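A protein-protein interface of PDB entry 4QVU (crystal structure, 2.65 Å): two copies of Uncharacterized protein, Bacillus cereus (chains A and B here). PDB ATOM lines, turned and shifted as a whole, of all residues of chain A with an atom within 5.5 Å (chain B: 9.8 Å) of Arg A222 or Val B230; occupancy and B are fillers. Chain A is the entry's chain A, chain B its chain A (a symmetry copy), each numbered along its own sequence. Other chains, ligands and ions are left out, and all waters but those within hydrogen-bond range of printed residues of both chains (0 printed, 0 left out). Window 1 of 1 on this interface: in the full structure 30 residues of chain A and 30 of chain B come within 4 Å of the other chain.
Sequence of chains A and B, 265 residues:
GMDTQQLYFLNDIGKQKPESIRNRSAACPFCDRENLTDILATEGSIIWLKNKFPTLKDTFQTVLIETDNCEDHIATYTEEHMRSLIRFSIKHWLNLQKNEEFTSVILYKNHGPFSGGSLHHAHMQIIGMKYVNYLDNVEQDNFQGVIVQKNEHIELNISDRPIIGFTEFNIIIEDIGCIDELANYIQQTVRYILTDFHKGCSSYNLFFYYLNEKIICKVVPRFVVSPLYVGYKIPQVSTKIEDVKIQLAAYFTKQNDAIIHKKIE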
ATOM      1  N   PHE A 114      27.008   2.607   3.382  1.00  0.00           N
ATOM      2  CA  PHE A 114      27.601   2.805   4.714  1.00  0.00           C
ATOM      3  C   PHE A 114      26.612   3.447   5.702  1.00  0.00           C
ATOM      4  O   PHE A 114      27.043   3.961   6.741  1.00  0.00           O
ATOM      5  CB  PHE A 114      28.877   3.656   4.622  1.00  0.00           C
ATOM      6  CG  PHE A 114      29.886   3.110   3.642  1.00  0.00           C
ATOM      7  CD1 PHE A 114      30.451   1.851   3.827  1.00  0.00           C
ATOM      8  CD2 PHE A 114      30.296   3.863   2.551  1.00  0.00           C
ATOM      9  CE1 PHE A 114      31.381   1.343   2.918  1.00  0.00           C
ATOM     10  CE2 PHE A 114      31.244   3.363   1.655  1.00  0.00           C
ATOM     11  CZ  PHE A 114      31.778   2.105   1.844  1.00  0.00           C
ATOM     12  N   SER A 115      25.294   3.336   5.423  1.00  0.00           N
ATOM     13  CA  SER A 115      24.219   3.878   6.264  1.00  0.00           C
ATOM     14  C   SER A 115      23.639   2.821   7.214  1.00  0.00           C
ATOM     15  O   SER A 115      23.154   3.174   8.289  1.00  0.00           O
ATOM     16  CB  SER A 115      23.096   4.457   5.402  1.00  0.00           C
ATOM     17  OG  SER A 115      22.534   3.502   4.516  1.00  0.00           O
ATOM     18  N   GLY A 116      23.694   1.554   6.806  1.00  0.00           N
ATOM     19  CA  GLY A 116      23.151   0.430   7.560  1.00  0.00           C
ATOM     20  C   GLY A 116      21.814  -0.072   7.035  1.00  0.00           C
ATOM     21  O   GLY A 116      21.104  -0.793   7.740  1.00  0.00           O
ATOM     22  N   ILE A 163      25.510  13.766  18.249  1.00  0.00           N
ATOM     23  CA  ILE A 163      25.160  12.555  18.979  1.00  0.00           C
ATOM     24  C   ILE A 163      26.329  11.567  18.930  1.00  0.00           C
ATOM     25  O   ILE A 163      26.666  11.000  19.967  1.00  0.00           O
ATOM     26  CB  ILE A 163      23.856  11.913  18.432  1.00  0.00           C
ATOM     27  CG1 ILE A 163      22.690  12.933  18.399  1.00  0.00           C
ATOM     28  CG2 ILE A 163      23.483  10.643  19.222  1.00  0.00           C
ATOM     29  CD1 ILE A 163      21.351  12.431  17.813  1.00  0.00           C
ATOM     30  N   ILE A 164      26.944  11.372  17.739  1.00  0.00           N
ATOM     31  CA  ILE A 164      28.004  10.379  17.522  1.00  0.00           C
ATOM     32  C   ILE A 164      29.405  11.021  17.509  1.00  0.00           C
ATOM     33  O   ILE A 164      30.353  10.325  17.850  1.00  0.00           O
ATOM     34  CB  ILE A 164      27.735   9.584  16.214  1.00  0.00           C
ATOM     35  CG1 ILE A 164      26.463   8.735  16.363  1.00  0.00           C
ATOM     36  CG2 ILE A 164      28.904   8.683  15.799  1.00  0.00           C
ATOM     37  CD1 ILE A 164      26.444   7.676  17.638  1.00  0.00           C
ATOM     38  N   GLU A 168      26.732  16.485  11.694  1.00  0.00           N
ATOM     39  CA  GLU A 168      25.281  16.323  11.818  1.00  0.00           C
ATOM     40  C   GLU A 168      24.629  17.648  11.502  1.00  0.00           C
ATOM     41  O   GLU A 168      24.982  18.660  12.108  1.00  0.00           O
ATOM     42  CB  GLU A 168      24.883  15.810  13.219  1.00  0.00           C
ATOM     43  CG  GLU A 168      25.437  14.424  13.529  1.00  0.00           C
ATOM     44  CD  GLU A 168      25.194  13.876  14.922  1.00  0.00           C
ATOM     45  OE1 GLU A 168      24.566  14.576  15.749  1.00  0.00           O
ATOM     46  OE2 GLU A 168      25.659  12.747  15.196  1.00  0.00           O
ATOM     47  N   CYS A 201      30.023  12.030  -0.830  1.00  0.00           N
ATOM     48  CA  CYS A 201      29.974  11.137   0.320  1.00  0.00           C
ATOM     49  C   CYS A 201      29.181   9.817   0.046  1.00  0.00           C
ATOM     50  O   CYS A 201      29.417   8.835   0.764  1.00  0.00           O
ATOM     51  CB  CYS A 201      29.393  11.879   1.514  1.00  0.00           C
ATOM     52  SG  CYS A 201      29.553  11.001   3.080  1.00  0.00           S
ATOM     53  N   SER A 202      28.278   9.781  -0.953  1.00  0.00           N
ATOM     54  CA  SER A 202      27.485   8.614  -1.417  1.00  0.00           C
ATOM     55  C   SER A 202      26.503   8.023  -0.359  1.00  0.00           C
ATOM     56  O   SER A 202      25.507   7.421  -0.772  1.00  0.00           O
ATOM     57  CB  SER A 202      28.382   7.475  -1.906  1.00  0.00           C
ATOM     58  OG  SER A 202      28.950   6.713  -0.851  1.00  0.00           O
ATOM     59  N   SER A 203      26.793   8.140   0.959  1.00  0.00           N
ATOM     60  CA  SER A 203      25.941   7.597   2.028  1.00  0.00           C
ATOM     61  C   SER A 203      25.532   8.650   3.057  1.00  0.00           C
ATOM     62  O   SER A 203      26.349   9.492   3.459  1.00  0.00           O
ATOM     63  CB  SER A 203      26.630   6.454   2.769  1.00  0.00           C
ATOM     64  OG  SER A 203      26.923   5.357   1.922  1.00  0.00           O
ATOM     65  N   TYR A 204      24.278   8.552   3.535  1.00  0.00           N
ATOM     66  CA  TYR A 204      23.742   9.429   4.568  1.00  0.00           C
ATOM     67  C   TYR A 204      22.553   8.785   5.253  1.00  0.00           C
ATOM     68  O   TYR A 204      21.994   7.795   4.772  1.00  0.00           O
ATOM     69  CB  TYR A 204      23.331  10.815   3.998  1.00  0.00           C
ATOM     70  CG  TYR A 204      22.150  10.790   3.045  1.00  0.00           C
ATOM     71  CD1 TYR A 204      20.849  10.941   3.510  1.00  0.00           C
ATOM     72  CD2 TYR A 204      22.339  10.649   1.671  1.00  0.00           C
ATOM     73  CE1 TYR A 204      19.761  10.917   2.642  1.00  0.00           C
ATOM     74  CE2 TYR A 204      21.261  10.641   0.790  1.00  0.00           C
ATOM     75  CZ  TYR A 204      19.970  10.776   1.280  1.00  0.00           C
ATOM     76  OH  TYR A 204      18.891  10.767   0.424  1.00  0.00           O
ATOM     77  N   ASN A 205      22.125   9.411   6.344  1.00  0.00           N
ATOM     78  CA  ASN A 205      20.938   9.055   7.097  1.00  0.00           C
ATOM     79  C   ASN A 205      20.088  10.265   7.364  1.00  0.00           C
ATOM     80  O   ASN A 205      20.622  11.362   7.575  1.00  0.00           O
ATOM     81  CB  ASN A 205      21.300   8.420   8.438  1.00  0.00           C
ATOM     82  CG  ASN A 205      21.831   7.020   8.437  1.00  0.00           C
ATOM     83  OD1 ASN A 205      22.915   6.775   8.932  1.00  0.00           O
ATOM     84  ND2 ASN A 205      21.034   6.052   8.044  1.00  0.00           N
ATOM     85  N   PHE A 207      17.143  11.409  10.154  1.00  0.00           N
ATOM     86  CA  PHE A 207      16.482  11.061  11.413  1.00  0.00           C
ATOM     87  C   PHE A 207      15.502  12.142  11.752  1.00  0.00           C
ATOM     88  O   PHE A 207      15.863  13.319  11.725  1.00  0.00           O
ATOM     89  CB  PHE A 207      17.459  10.836  12.571  1.00  0.00           C
ATOM     90  CG  PHE A 207      18.493   9.778  12.308  1.00  0.00           C
ATOM     91  CD1 PHE A 207      18.153   8.431  12.325  1.00  0.00           C
ATOM     92  CD2 PHE A 207      19.813  10.126  12.052  1.00  0.00           C
ATOM     93  CE1 PHE A 207      19.103   7.454  12.063  1.00  0.00           C
ATOM     94  CE2 PHE A 207      20.766   9.147  11.807  1.00  0.00           C
ATOM     95  CZ  PHE A 207      20.404   7.818  11.813  1.00  0.00           C
ATOM     96  N   TYR A 209      12.634  13.780  14.474  1.00  0.00           N
ATOM     97  CA  TYR A 209      12.306  13.921  15.895  1.00  0.00           C
ATOM     98  C   TYR A 209      11.170  14.918  16.092  1.00  0.00           C
ATOM     99  O   TYR A 209      11.095  15.925  15.375  1.00  0.00           O
ATOM    100  CB  TYR A 209      13.538  14.393  16.717  1.00  0.00           C
ATOM    101  CG  TYR A 209      14.857  13.723  16.374  1.00  0.00           C
ATOM    102  CD1 TYR A 209      15.597  14.120  15.263  1.00  0.00           C
ATOM    103  CD2 TYR A 209      15.413  12.758  17.215  1.00  0.00           C
ATOM    104  CE1 TYR A 209      16.804  13.510  14.939  1.00  0.00           C
ATOM    105  CE2 TYR A 209      16.646  12.172  16.927  1.00  0.00           C
ATOM    106  CZ  TYR A 209      17.326  12.536  15.775  1.00  0.00           C
ATOM    107  OH  TYR A 209      18.539  11.976  15.468  1.00  0.00           O
ATOM    108  N   VAL A 220      22.705  13.138   8.499  1.00  0.00           N
ATOM    109  CA  VAL A 220      24.008  12.658   8.958  1.00  0.00           C
ATOM    110  C   VAL A 220      24.795  11.987   7.810  1.00  0.00           C
ATOM    111  O   VAL A 220      24.423  10.885   7.400  1.00  0.00           O
ATOM    112  CB  VAL A 220      23.844  11.660  10.159  1.00  0.00           C
ATOM    113  CG1 VAL A 220      25.195  11.257  10.750  1.00  0.00           C
ATOM    114  CG2 VAL A 220      22.931  12.221  11.250  1.00  0.00           C
ATOM    115  N   PRO A 221      25.916  12.586   7.316  1.00  0.00           N
ATOM    116  CA  PRO A 221      26.742  11.878   6.327  1.00  0.00           C
ATOM    117  C   PRO A 221      27.359  10.617   6.938  1.00  0.00           C
ATOM    118  O   PRO A 221      27.675  10.580   8.135  1.00  0.00           O
ATOM    119  CB  PRO A 221      27.820  12.899   5.951  1.00  0.00           C
ATOM    120  CG  PRO A 221      27.349  14.206   6.501  1.00  0.00           C
ATOM    121  CD  PRO A 221      26.534  13.872   7.693  1.00  0.00           C
ATOM    122  N   ARG A 222      27.464   9.563   6.128  1.00  0.00           N
ATOM    123  CA  ARG A 222      28.011   8.290   6.558  1.00  0.00           C
ATOM    124  C   ARG A 222      29.127   7.916   5.599  1.00  0.00           C
ATOM    125  O   ARG A 222      28.952   7.928   4.382  1.00  0.00           O
ATOM    126  CB  ARG A 222      26.902   7.223   6.631  1.00  0.00           C
ATOM    127  CG  ARG A 222      25.753   7.507   7.617  1.00  0.00           C
ATOM    128  CD  ARG A 222      26.112   7.452   9.105  1.00  0.00           C
ATOM    129  NE  ARG A 222      26.685   6.156   9.490  1.00  0.00           N
ATOM    130  CZ  ARG A 222      25.995   5.122   9.957  1.00  0.00           C
ATOM    131  NH1 ARG A 222      24.688   5.216  10.142  1.00  0.00           N
ATOM    132  NH2 ARG A 222      26.611   3.992  10.265  1.00  0.00           N
ATOM    133  N   PHE A 223      30.301   7.673   6.148  1.00  0.00           N
ATOM    134  CA  PHE A 223      31.525   7.383   5.386  1.00  0.00           C
ATOM    135  C   PHE A 223      32.478   6.560   6.228  1.00  0.00           C
ATOM    136  O   PHE A 223      32.427   6.632   7.460  1.00  0.00           O
ATOM    137  CB  PHE A 223      32.210   8.707   4.927  1.00  0.00           C
ATOM    138  CG  PHE A 223      32.386   9.738   6.020  1.00  0.00           C
ATOM    139  CD1 PHE A 223      31.360  10.626   6.335  1.00  0.00           C
ATOM    140  CD2 PHE A 223      33.565   9.803   6.756  1.00  0.00           C
ATOM    141  CE1 PHE A 223      31.499  11.545   7.386  1.00  0.00           C
ATOM    142  CE2 PHE A 223      33.713  10.738   7.794  1.00  0.00           C
ATOM    143  CZ  PHE A 223      32.675  11.601   8.102  1.00  0.00           C
ATOM    144  N   VAL A 224      33.343   5.779   5.578  1.00  0.00           N
ATOM    145  CA  VAL A 224      34.355   5.026   6.316  1.00  0.00           C
ATOM    146  C   VAL A 224      35.427   6.053   6.693  1.00  0.00           C
ATOM    147  O   VAL A 224      35.987   6.719   5.816  1.00  0.00           O
ATOM    148  CB  VAL A 224      34.899   3.785   5.544  1.00  0.00           C
ATOM    149  CG1 VAL A 224      36.032   3.106   6.309  1.00  0.00           C
ATOM    150  CG2 VAL A 224      33.777   2.786   5.258  1.00  0.00           C
ATOM    151  N   PHE B 114      35.653  -2.321   6.003  1.00  0.00           N
ATOM    152  CA  PHE B 114      35.243  -1.107   6.725  1.00  0.00           C
ATOM    153  C   PHE B 114      36.392  -0.503   7.550  1.00  0.00           C
ATOM    154  O   PHE B 114      36.133   0.311   8.443  1.00  0.00           O
ATOM    155  CB  PHE B 114      34.039  -1.395   7.636  1.00  0.00           C
ATOM    156  CG  PHE B 114      32.878  -2.024   6.906  1.00  0.00           C
ATOM    157  CD1 PHE B 114      32.237  -1.351   5.870  1.00  0.00           C
ATOM    158  CD2 PHE B 114      32.404  -3.276   7.272  1.00  0.00           C
ATOM    159  CE1 PHE B 114      31.167  -1.935   5.190  1.00  0.00           C
ATOM    160  CE2 PHE B 114      31.318  -3.849   6.607  1.00  0.00           C
ATOM    161  CZ  PHE B 114      30.708  -3.175   5.570  1.00  0.00           C
ATOM    162  N   PHE B 166      34.371   4.677  20.386  1.00  0.00           N
ATOM    163  CA  PHE B 166      33.767   3.348  20.399  1.00  0.00           C
ATOM    164  C   PHE B 166      34.700   2.395  21.152  1.00  0.00           C
ATOM    165  O   PHE B 166      35.289   2.820  22.145  1.00  0.00           O
ATOM    166  CB  PHE B 166      33.438   2.886  18.970  1.00  0.00           C
ATOM    167  CG  PHE B 166      32.308   3.687  18.357  1.00  0.00           C
ATOM    168  CD1 PHE B 166      30.978   3.322  18.564  1.00  0.00           C
ATOM    169  CD2 PHE B 166      32.568   4.824  17.597  1.00  0.00           C
ATOM    170  CE1 PHE B 166      29.934   4.059  18.001  1.00  0.00           C
ATOM    171  CE2 PHE B 166      31.515   5.576  17.046  1.00  0.00           C
ATOM    172  CZ  PHE B 166      30.209   5.186  17.249  1.00  0.00           C
ATOM    173  N   PHE B 223      33.145  -1.312  12.073  1.00  0.00           N
ATOM    174  CA  PHE B 223      31.819  -1.814  11.683  1.00  0.00           C
ATOM    175  C   PHE B 223      30.908  -0.655  11.329  1.00  0.00           C
ATOM    176  O   PHE B 223      31.113   0.458  11.821  1.00  0.00           O
ATOM    177  CB  PHE B 223      31.195  -2.662  12.834  1.00  0.00           C
ATOM    178  CG  PHE B 223      31.237  -2.005  14.196  1.00  0.00           C
ATOM    179  CD1 PHE B 223      32.363  -2.118  15.009  1.00  0.00           C
ATOM    180  CD2 PHE B 223      30.164  -1.248  14.657  1.00  0.00           C
ATOM    181  CE1 PHE B 223      32.427  -1.463  16.247  1.00  0.00           C
ATOM    182  CE2 PHE B 223      30.220  -0.610  15.907  1.00  0.00           C
ATOM    183  CZ  PHE B 223      31.354  -0.721  16.692  1.00  0.00           C
ATOM    184  N   VAL B 224      29.910  -0.905  10.479  1.00  0.00           N
ATOM    185  CA  VAL B 224      28.935   0.135  10.160  1.00  0.00           C
ATOM    186  C   VAL B 224      28.006   0.202  11.375  1.00  0.00           C
ATOM    187  O   VAL B 224      27.401  -0.807  11.753  1.00  0.00           O
ATOM    188  CB  VAL B 224      28.202  -0.088   8.803  1.00  0.00           C
ATOM    189  CG1 VAL B 224      27.118   0.961   8.576  1.00  0.00           C
ATOM    190  CG2 VAL B 224      29.196  -0.085   7.639  1.00  0.00           C
ATOM    191  N   VAL B 225      27.993   1.350  12.054  1.00  0.00           N
ATOM    192  CA  VAL B 225      27.167   1.541  13.255  1.00  0.00           C
ATOM    193  C   VAL B 225      25.680   1.494  12.842  1.00  0.00           C
ATOM    194  O   VAL B 225      25.313   1.999  11.770  1.00  0.00           O
ATOM    195  CB  VAL B 225      27.525   2.858  14.014  1.00  0.00           C
ATOM    196  CG1 VAL B 225      26.762   2.969  15.328  1.00  0.00           C
ATOM    197  CG2 VAL B 225      29.033   2.955  14.270  1.00  0.00           C
ATOM    198  N   SER B 226      24.850   0.834  13.682  1.00  0.00           N
ATOM    199  CA  SER B 226      23.402   0.707  13.526  1.00  0.00           C
ATOM    200  C   SER B 226      22.733   2.109  13.409  1.00  0.00           C
ATOM    201  O   SER B 226      23.051   3.003  14.203  1.00  0.00           O
ATOM    202  CB  SER B 226      22.818  -0.067  14.706  1.00  0.00           C
ATOM    203  OG  SER B 226      21.403   0.037  14.780  1.00  0.00           O
ATOM    204  N   PRO B 227      21.807   2.311  12.441  1.00  0.00           N
ATOM    205  CA  PRO B 227      21.162   3.628  12.293  1.00  0.00           C
ATOM    206  C   PRO B 227      20.375   4.071  13.530  1.00  0.00           C
ATOM    207  O   PRO B 227      20.294   5.267  13.799  1.00  0.00           O
ATOM    208  CB  PRO B 227      20.209   3.425  11.118  1.00  0.00           C
ATOM    209  CG  PRO B 227      20.730   2.267  10.394  1.00  0.00           C
ATOM    210  CD  PRO B 227      21.329   1.369  11.414  1.00  0.00           C
ATOM    211  N   LEU B 228      19.812   3.116  14.287  1.00  0.00           N
ATOM    212  CA  LEU B 228      19.032   3.396  15.489  1.00  0.00           C
ATOM    213  C   LEU B 228      19.934   3.888  16.599  1.00  0.00           C
ATOM    214  O   LEU B 228      19.480   4.663  17.430  1.00  0.00           O
ATOM    215  CB  LEU B 228      18.241   2.165  15.931  1.00  0.00           C
ATOM    216  CG  LEU B 228      16.794   2.132  15.456  1.00  0.00           C
ATOM    217  CD1 LEU B 228      16.683   2.239  13.936  1.00  0.00           C
ATOM    218  CD2 LEU B 228      16.078   0.915  15.978  1.00  0.00           C
ATOM    219  N   TYR B 229      21.219   3.506  16.569  1.00  0.00           N
ATOM    220  CA  TYR B 229      22.211   3.969  17.521  1.00  0.00           C
ATOM    221  C   TYR B 229      22.737   5.345  17.091  1.00  0.00           C
ATOM    222  O   TYR B 229      22.857   6.237  17.935  1.00  0.00           O
ATOM    223  CB  TYR B 229      23.375   2.962  17.684  1.00  0.00           C
ATOM    224  CG  TYR B 229      24.276   3.337  18.840  1.00  0.00           C
ATOM    225  CD1 TYR B 229      23.938   3.000  20.147  1.00  0.00           C
ATOM    226  CD2 TYR B 229      25.393   4.146  18.647  1.00  0.00           C
ATOM    227  CE1 TYR B 229      24.714   3.410  21.227  1.00  0.00           C
ATOM    228  CE2 TYR B 229      26.172   4.571  19.721  1.00  0.00           C
ATOM    229  CZ  TYR B 229      25.834   4.190  21.010  1.00  0.00           C
ATOM    230  OH  TYR B 229      26.592   4.577  22.089  1.00  0.00           O
ATOM    231  N   VAL B 230      23.057   5.521  15.792  1.00  0.00           N
ATOM    232  CA  VAL B 230      23.582   6.784  15.243  1.00  0.00           C
ATOM    233  C   VAL B 230      22.613   7.947  15.529  1.00  0.00           C
ATOM    234  O   VAL B 230      23.050   8.986  16.026  1.00  0.00           O
ATOM    235  CB  VAL B 230      23.892   6.689  13.729  1.00  0.00           C
ATOM    236  CG1 VAL B 230      24.085   8.063  13.101  1.00  0.00           C
ATOM    237  CG2 VAL B 230      25.111   5.818  13.486  1.00  0.00           C
ATOM    238  N   GLY B 231      21.328   7.754  15.257  1.00  0.00           N
ATOM    239  CA  GLY B 231      20.346   8.819  15.438  1.00  0.00           C
ATOM    240  C   GLY B 231      19.634   8.885  16.768  1.00  0.00           C
ATOM    241  O   GLY B 231      19.122   9.945  17.131  1.00  0.00           O
ATOM    242  N   TYR B 232      19.559   7.763  17.501  1.00  0.00           N
ATOM    243  CA  TYR B 232      18.776   7.767  18.734  1.00  0.00           C
ATOM    244  C   TYR B 232      19.469   7.080  19.913  1.00  0.00           C
ATOM    245  O   TYR B 232      18.851   6.977  20.976  1.00  0.00           O
ATOM    246  CB  TYR B 232      17.433   7.056  18.480  1.00  0.00           C
ATOM    247  CG  TYR B 232      16.683   7.559  17.265  1.00  0.00           C
ATOM    248  CD1 TYR B 232      15.921   8.723  17.323  1.00  0.00           C
ATOM    249  CD2 TYR B 232      16.716   6.859  16.060  1.00  0.00           C
ATOM    250  CE1 TYR B 232      15.216   9.182  16.210  1.00  0.00           C
ATOM    251  CE2 TYR B 232      16.007   7.305  14.944  1.00  0.00           C
ATOM    252  CZ  TYR B 232      15.265   8.472  15.023  1.00  0.00           C
ATOM    253  OH  TYR B 232      14.556   8.924  13.937  1.00  0.00           O
ATOM    254  N   LYS B 233      20.725   6.633  19.750  1.00  0.00           N
ATOM    255  CA  LYS B 233      21.483   5.906  20.783  1.00  0.00           C
ATOM    256  C   LYS B 233      20.623   4.749  21.388  1.00  0.00           C
ATOM    257  O   LYS B 233      20.591   4.548  22.606  1.00  0.00           O
ATOM    258  CB  LYS B 233      22.019   6.850  21.878  1.00  0.00           C
ATOM    259  CG  LYS B 233      23.343   7.483  21.481  1.00  0.00           C
ATOM    260  CD  LYS B 233      23.801   8.495  22.491  1.00  0.00           C
ATOM    261  CE  LYS B 233      25.235   8.882  22.237  1.00  0.00           C
ATOM    262  NZ  LYS B 233      25.607  10.133  22.952  1.00  0.00           N
ATOM    263  N   ILE B 234      19.937   4.000  20.501  1.00  0.00           N
ATOM    264  CA  ILE B 234      19.162   2.807  20.803  1.00  0.00           C
ATOM    265  C   ILE B 234      20.060   1.644  20.404  1.00  0.00           C
ATOM    266  O   ILE B 234      20.232   1.402  19.205  1.00  0.00           O
ATOM    267  CB  ILE B 234      17.748   2.777  20.131  1.00  0.00           C
ATOM    268  CG1 ILE B 234      16.863   3.937  20.647  1.00  0.00           C
ATOM    269  CG2 ILE B 234      17.072   1.411  20.368  1.00  0.00           C
ATOM    270  CD1 ILE B 234      15.551   4.130  19.963  1.00  0.00           C
ATOM    271  N   PRO B 235      20.719   0.966  21.370  1.00  0.00           N
ATOM    272  CA  PRO B 235      21.639  -0.122  20.986  1.00  0.00           C
ATOM    273  C   PRO B 235      20.923  -1.434  20.716  1.00  0.00           C
ATOM    274  O   PRO B 235      19.861  -1.688  21.282  1.00  0.00           O
ATOM    275  CB  PRO B 235      22.553  -0.251  22.199  1.00  0.00           C
ATOM    276  CG  PRO B 235      21.701   0.184  23.367  1.00  0.00           C
ATOM    277  CD  PRO B 235      20.657   1.139  22.840  1.00  0.00           C
ATOM    278  N   GLN B 236      21.523  -2.272  19.855  1.00  0.00           N
ATOM    279  CA  GLN B 236      21.010  -3.612  19.521  1.00  0.00           C
ATOM    280  C   GLN B 236      21.584  -4.603  20.534  1.00  0.00           C
ATOM    281  O   GLN B 236      20.840  -5.367  21.151  1.00  0.00           O
ATOM    282  CB  GLN B 236      21.355  -4.022  18.067  1.00  0.00           C
ATOM    283  CG  GLN B 236      21.109  -2.953  16.979  1.00  0.00           C
ATOM    284  CD  GLN B 236      19.689  -2.421  16.860  1.00  0.00           C
ATOM    285  OE1 GLN B 236      19.462  -1.202  16.854  1.00  0.00           O
ATOM    286  NE2 GLN B 236      18.709  -3.308  16.746  1.00  0.00           N
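Printed residues of chain B within 4 Å of Phe A114: Phe B114 (3.99 Å) and Val B224 (3.5 Å).
Of the printed residues of chain B, Ser A115 touches Pro B227 (3.3 Å).
Printed residues of chain B within 4 Å of Ile A164: Tyr B229 (3.7 Å) and Val B230 (3.4 Å).
Arg A222 touches just these residues of chain B: Val B224 (3.5 Å), Val B225 (2.8 Å) and Val B230 (3.4 Å).
Of the printed residues of chain A, Val B224 touches Phe A114 (3.5 Å), Gly A116 (3.9 Å) and Arg A222 (3.5 Å).
Printed residues of chain A within 4 Å of Val B225: Arg A222.
Leu B228 touches none of the printed residues of chain A.
Val B230 touches just these residues of chain A: Ile A163, Ile A164, Phe A207 and Arg A222.
The nearest residue of chain B that does not touch Arg A222 is Pro B227 (4.4 Å).
The nearest residue of chain A that does not touch Val B230 is Val A220 (4.1 Å).
The nearest printed residue of chain A that does not touch Tyr B229 is Ile A163 (4.6 Å).
Phe A114 touches its own counterpart, Phe B114.
Phe A114 touches Val B224, and with the chains exchanged Val A224 touches Phe B114.
Of the 19 pairs that touch across the chains among the printed residues, 3 have their exchanged pair printed and touching as well.
The backbone NH of Ile A164 sits at hydrogen-bond distance from the side-chain carboxylate of Glu A168.
The side-chain amide oxygen of Asn A205 lies within hydrogen-bond range of the guanidinium group of Arg A222 (2.7 Å).
The backbone NH (N) of Phe A114 sits at hydrogen-bond distance from the side-chain hydroxyl (OG) of Ser A203 (3.1 Å).
N of Lys B233 sits at hydrogen-bond distance from O of Leu B228 (3.3 Å).
N of Ile A163 is in hydrogen-bond range of OE1 of Glu A168 (2.8 Å).
NH1 of Arg A222 lies within hydrogen-bond range of O of Ser A115 (3.2 Å).
Phe A114 touches Phe B114.
Val B224 touches Gly A116 (CG1 to N, 3.9 Å).
O of Val B230 touches CG2 of Ile A163 (3.6 Å).
Val B230 touches Ile A164.
Phe A207 touches Pro B227.
Gly B231 touches Phe A207 (N to CZ, 3.6 Å).
Phe A207 touches Tyr B232 (CD1 to CE2, 3.6 Å).
Tyr A209 touches Tyr B232.
Arg A222 touches Val B224.
Val A224 touches Phe B114 (CG1 to O, 3.5 Å).
Hydrophobic or aromatic side chains of chain B that line the printed part of chain A: Phe B114, Val B224, Pro B227, Tyr B229, Val B230 and Tyr B232.
Of the 18 printed residues of chain A, 9 touch a printed residue of chain B.
Among the printed residues, 19 pairs touch across the chains.
The guanidinium group (NH2) of Arg A222 is in hydrogen-bond range of the backbone carbonyl oxygen (O) of Val B225, at 2.8 Å.
The backbone carbonyl oxygen (O) of Ile A163 sits at hydrogen-bond distance from the side-chain amino group (NZ) of Lys B233 (3.3 Å).
OH of Tyr A209 sits at hydrogen-bond distance from O of Gly B231 (2.7 Å).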
